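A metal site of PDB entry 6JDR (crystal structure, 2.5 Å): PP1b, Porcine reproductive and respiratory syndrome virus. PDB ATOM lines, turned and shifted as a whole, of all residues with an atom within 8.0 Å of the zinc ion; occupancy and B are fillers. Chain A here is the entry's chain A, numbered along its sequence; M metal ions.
The backbone carbonyl oxygen (O) of Cys 53 sits at hydrogen-bond distance from the backbone NH (N) of Gly 48 (2.8 Å).
The side-chain sulfur (SG) of Cys 53 sits close to the backbone NH (N) of Ser 49, 3.0 Å away.
The backbone NH (N) of Ser 47 is in hydrogen-bond range of the backbone carbonyl oxygen (O) of Cys 53 (3.2 Å).
The backbone carbonyl oxygen (O) of Cys 53 sits close to the backbone NH (N) of Gly 46 (3.3 Å).
The backbone NH (N) of Glu 52 lies close to the side-chain sulfur (SG) of Cys 50 (3.2 Å).
Within 4 Å of the zinc ion: Cys 41, His 43, Cys 50 and Cys 53.
The nearest printed residue that does not touch the zinc ion is Glu 52 (4.4 Å).
SG of Cys 41 is bound to the zinc ion, 2.1 Å away.
A ring nitrogen (ND1) of His 43 binds the zinc ion (2.3 Å).
The side-chain sulfur (SG) of Cys 50 is bound to the zinc ion (2.4 Å).
The zinc ion is bound by the side-chain sulfur (SG) of Cys 53 (2.5 Å).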
ATOM      1  N   ILE A  39     -16.060 -27.850 -22.990  1.00  0.00           N
ATOM      2  CA  ILE A  39     -15.417 -27.760 -21.674  1.00  0.00           C
ATOM      3  C   ILE A  39     -15.815 -26.477 -20.941  1.00  0.00           C
ATOM      4  O   ILE A  39     -16.615 -25.676 -21.430  1.00  0.00           O
ATOM      5  CB  ILE A  39     -13.870 -27.903 -21.780  1.00  0.00           C
ATOM      6  CG1 ILE A  39     -13.248 -26.824 -22.672  1.00  0.00           C
ATOM      7  CG2 ILE A  39     -13.519 -29.279 -22.307  1.00  0.00           C
ATOM      8  CD1 ILE A  39     -11.758 -26.704 -22.478  1.00  0.00           C
ATOM      9  N   TRP A  40     -15.268 -26.320 -19.732  1.00  0.00           N
ATOM     10  CA  TRP A  40     -15.568 -25.212 -18.808  1.00  0.00           C
ATOM     11  C   TRP A  40     -15.680 -23.811 -19.416  1.00  0.00           C
ATOM     12  O   TRP A  40     -16.497 -23.029 -18.967  1.00  0.00           O
ATOM     13  CB  TRP A  40     -14.570 -25.217 -17.628  1.00  0.00           C
ATOM     14  CG  TRP A  40     -13.123 -25.402 -18.000  1.00  0.00           C
ATOM     15  CD1 TRP A  40     -12.204 -24.424 -18.217  1.00  0.00           C
ATOM     16  CD2 TRP A  40     -12.431 -26.642 -18.171  1.00  0.00           C
ATOM     17  NE1 TRP A  40     -10.982 -24.973 -18.527  1.00  0.00           N
ATOM     18  CE2 TRP A  40     -11.093 -26.341 -18.508  1.00  0.00           C
ATOM     19  CE3 TRP A  40     -12.810 -27.995 -18.092  1.00  0.00           C
ATOM     20  CZ2 TRP A  40     -10.129 -27.326 -18.759  1.00  0.00           C
ATOM     21  CZ3 TRP A  40     -11.859 -28.972 -18.344  1.00  0.00           C
ATOM     22  CH2 TRP A  40     -10.530 -28.629 -18.669  1.00  0.00           C
ATOM     23  N   CYS A  41     -14.875 -23.492 -20.427  1.00  0.00           N
ATOM     24  CA  CYS A  41     -14.970 -22.170 -21.079  1.00  0.00           C
ATOM     25  C   CYS A  41     -16.120 -22.053 -22.098  1.00  0.00           C
ATOM     26  O   CYS A  41     -16.279 -21.010 -22.739  1.00  0.00           O
ATOM     27  CB  CYS A  41     -13.646 -21.822 -21.764  1.00  0.00           C
ATOM     28  SG  CYS A  41     -13.221 -22.858 -23.187  1.00  0.00           S
ATOM     29  N   GLY A  42     -16.909 -23.109 -22.244  1.00  0.00           N
ATOM     30  CA  GLY A  42     -18.078 -23.085 -23.130  1.00  0.00           C
ATOM     31  C   GLY A  42     -17.767 -23.345 -24.591  1.00  0.00           C
ATOM     32  O   GLY A  42     -18.629 -23.181 -25.449  1.00  0.00           O
ATOM     33  N   HIS A  43     -16.531 -23.738 -24.884  1.00  0.00           N
ATOM     34  CA  HIS A  43     -16.115 -24.066 -26.250  1.00  0.00           C
ATOM     35  C   HIS A  43     -15.610 -25.517 -26.290  1.00  0.00           C
ATOM     36  O   HIS A  43     -15.398 -26.128 -25.234  1.00  0.00           O
ATOM     37  CB  HIS A  43     -15.010 -23.115 -26.718  1.00  0.00           C
ATOM     38  CG  HIS A  43     -15.377 -21.671 -26.637  1.00  0.00           C
ATOM     39  ND1 HIS A  43     -14.711 -20.777 -25.828  1.00  0.00           N
ATOM     40  CD2 HIS A  43     -16.341 -20.953 -27.259  1.00  0.00           C
ATOM     41  CE1 HIS A  43     -15.246 -19.583 -25.956  1.00  0.00           C
ATOM     42  NE2 HIS A  43     -16.242 -19.666 -26.819  1.00  0.00           N
ATOM     43  N   PRO A  44     -15.426 -26.073 -27.500  1.00  0.00           N
ATOM     44  CA  PRO A  44     -14.840 -27.409 -27.597  1.00  0.00           C
ATOM     45  C   PRO A  44     -13.368 -27.411 -27.212  1.00  0.00           C
ATOM     46  O   PRO A  44     -12.604 -26.529 -27.631  1.00  0.00           O
ATOM     47  CB  PRO A  44     -14.995 -27.757 -29.086  1.00  0.00           C
ATOM     48  CG  PRO A  44     -16.061 -26.851 -29.595  1.00  0.00           C
ATOM     49  CD  PRO A  44     -15.882 -25.584 -28.813  1.00  0.00           C
ATOM     50  N   ALA A  45     -12.956 -28.397 -26.423  1.00  0.00           N
ATOM     51  CA  ALA A  45     -11.559 -28.563 -26.071  1.00  0.00           C
ATOM     52  C   ALA A  45     -10.704 -28.553 -27.342  1.00  0.00           C
ATOM     53  O   ALA A  45     -11.043 -29.228 -28.316  1.00  0.00           O
ATOM     54  CB  ALA A  45     -11.339 -29.861 -25.313  1.00  0.00           C
ATOM     55  N   GLY A  46      -9.644 -27.751 -27.326  1.00  0.00           N
ATOM     56  CA  GLY A  46      -8.713 -27.679 -28.458  1.00  0.00           C
ATOM     57  C   GLY A  46      -9.170 -26.821 -29.628  1.00  0.00           C
ATOM     58  O   GLY A  46      -8.503 -26.783 -30.647  1.00  0.00           O
ATOM     59  N   SER A  47     -10.303 -26.134 -29.473  1.00  0.00           N
ATOM     60  CA  SER A  47     -10.856 -25.327 -30.569  1.00  0.00           C
ATOM     61  C   SER A  47     -10.116 -24.001 -30.769  1.00  0.00           C
ATOM     62  O   SER A  47     -10.095 -23.467 -31.872  1.00  0.00           O
ATOM     63  CB  SER A  47     -12.337 -25.041 -30.321  1.00  0.00           C
ATOM     64  OG  SER A  47     -12.534 -24.493 -29.038  1.00  0.00           O
ATOM     65  N   GLY A  48      -9.528 -23.471 -29.694  1.00  0.00           N
ATOM     66  CA  GLY A  48      -8.888 -22.159 -29.737  1.00  0.00           C
ATOM     67  C   GLY A  48      -9.863 -21.016 -30.002  1.00  0.00           C
ATOM     68  O   GLY A  48      -9.502 -20.019 -30.617  1.00  0.00           O
ATOM     69  N   SER A  49     -11.114 -21.187 -29.563  1.00  0.00           N
ATOM     70  CA  SER A  49     -12.118 -20.136 -29.685  1.00  0.00           C
ATOM     71  C   SER A  49     -11.842 -19.034 -28.662  1.00  0.00           C
ATOM     72  O   SER A  49     -12.111 -17.857 -28.901  1.00  0.00           O
ATOM     73  CB  SER A  49     -13.521 -20.698 -29.443  1.00  0.00           C
ATOM     74  OG  SER A  49     -13.752 -21.844 -30.241  1.00  0.00           O
ATOM     75  N   CYS A  50     -11.322 -19.447 -27.510  1.00  0.00           N
ATOM     76  CA  CYS A  50     -10.783 -18.536 -26.519  1.00  0.00           C
ATOM     77  C   CYS A  50      -9.445 -19.091 -26.040  1.00  0.00           C
ATOM     78  O   CYS A  50      -9.038 -20.168 -26.470  1.00  0.00           O
ATOM     79  CB  CYS A  50     -11.758 -18.379 -25.356  1.00  0.00           C
ATOM     80  SG  CYS A  50     -11.640 -19.682 -24.114  1.00  0.00           S
ATOM     81  N   SER A  51      -8.782 -18.371 -25.151  1.00  0.00           N
ATOM     82  CA  SER A  51      -7.450 -18.780 -24.674  1.00  0.00           C
ATOM     83  C   SER A  51      -7.484 -20.021 -23.782  1.00  0.00           C
ATOM     84  O   SER A  51      -6.477 -20.706 -23.639  1.00  0.00           O
ATOM     85  CB  SER A  51      -6.733 -17.620 -23.966  1.00  0.00           C
ATOM     86  OG  SER A  51      -7.543 -17.050 -22.948  1.00  0.00           O
ATOM     87  N   GLU A  52      -8.642 -20.317 -23.203  1.00  0.00           N
ATOM     88  CA  GLU A  52      -8.798 -21.489 -22.336  1.00  0.00           C
ATOM     89  C   GLU A  52      -8.872 -22.802 -23.119  1.00  0.00           C
ATOM     90  O   GLU A  52      -8.491 -23.856 -22.601  1.00  0.00           O
ATOM     91  CB  GLU A  52     -10.051 -21.331 -21.457  1.00  0.00           C
ATOM     92  CG  GLU A  52     -10.129 -22.325 -20.303  1.00  0.00           C
ATOM     93  CD  GLU A  52      -8.972 -22.193 -19.319  1.00  0.00           C
ATOM     94  OE1 GLU A  52      -8.625 -21.047 -18.953  1.00  0.00           O
ATOM     95  OE2 GLU A  52      -8.425 -23.239 -18.917  1.00  0.00           O
ATOM     96  N   CYS A  53      -9.364 -22.729 -24.359  1.00  0.00           N
ATOM     97  CA  CYS A  53      -9.476 -23.911 -25.222  1.00  0.00           C
ATOM     98  C   CYS A  53      -8.379 -23.953 -26.299  1.00  0.00           C
ATOM     99  O   CYS A  53      -8.537 -24.623 -27.327  1.00  0.00           O
ATOM    100  CB  CYS A  53     -10.863 -23.947 -25.877  1.00  0.00           C
ATOM    101  SG  CYS A  53     -11.307 -22.465 -26.827  1.00  0.00           S
ATOM    102  N   GLU A  54      -7.272 -23.239 -26.069  1.00  0.00           N
ATOM    103  CA  GLU A  54      -6.133 -23.246 -26.991  1.00  0.00           C
ATOM    104  C   GLU A  54      -5.236 -24.486 -26.877  1.00  0.00           C
ATOM    105  O   GLU A  54      -4.668 -24.916 -27.883  1.00  0.00           O
ATOM    106  CB  GLU A  54      -5.285 -21.974 -26.842  1.00  0.00           C
ATOM    107  CG  GLU A  54      -5.776 -20.814 -27.710  1.00  0.00           C
ATOM    108  CD  GLU A  54      -5.063 -19.505 -27.425  1.00  0.00           C
ATOM    109  OE1 GLU A  54      -3.927 -19.534 -26.907  1.00  0.00           O
ATOM    110  OE2 GLU A  54      -5.657 -18.447 -27.716  1.00  0.00           O
ATOM    111  N   PRO A  55      -5.076 -25.055 -25.666  1.00  0.00           N
ATOM    112  CA  PRO A  55      -4.285 -26.294 -25.572  1.00  0.00           C
ATOM    113  C   PRO A  55      -4.830 -27.374 -26.504  1.00  0.00           C
ATOM    114  O   PRO A  55      -6.026 -27.662 -26.469  1.00  0.00           O
ATOM    115  CB  PRO A  55      -4.448 -26.702 -24.106  1.00  0.00           C
ATOM    116  CG  PRO A  55      -4.710 -25.428 -23.384  1.00  0.00           C
ATOM    117  CD  PRO A  55      -5.494 -24.566 -24.336  1.00  0.00           C
HETATM  118 ZN    ZN M   1     -12.745 -21.661 -24.903  1.00  0.00          ZN
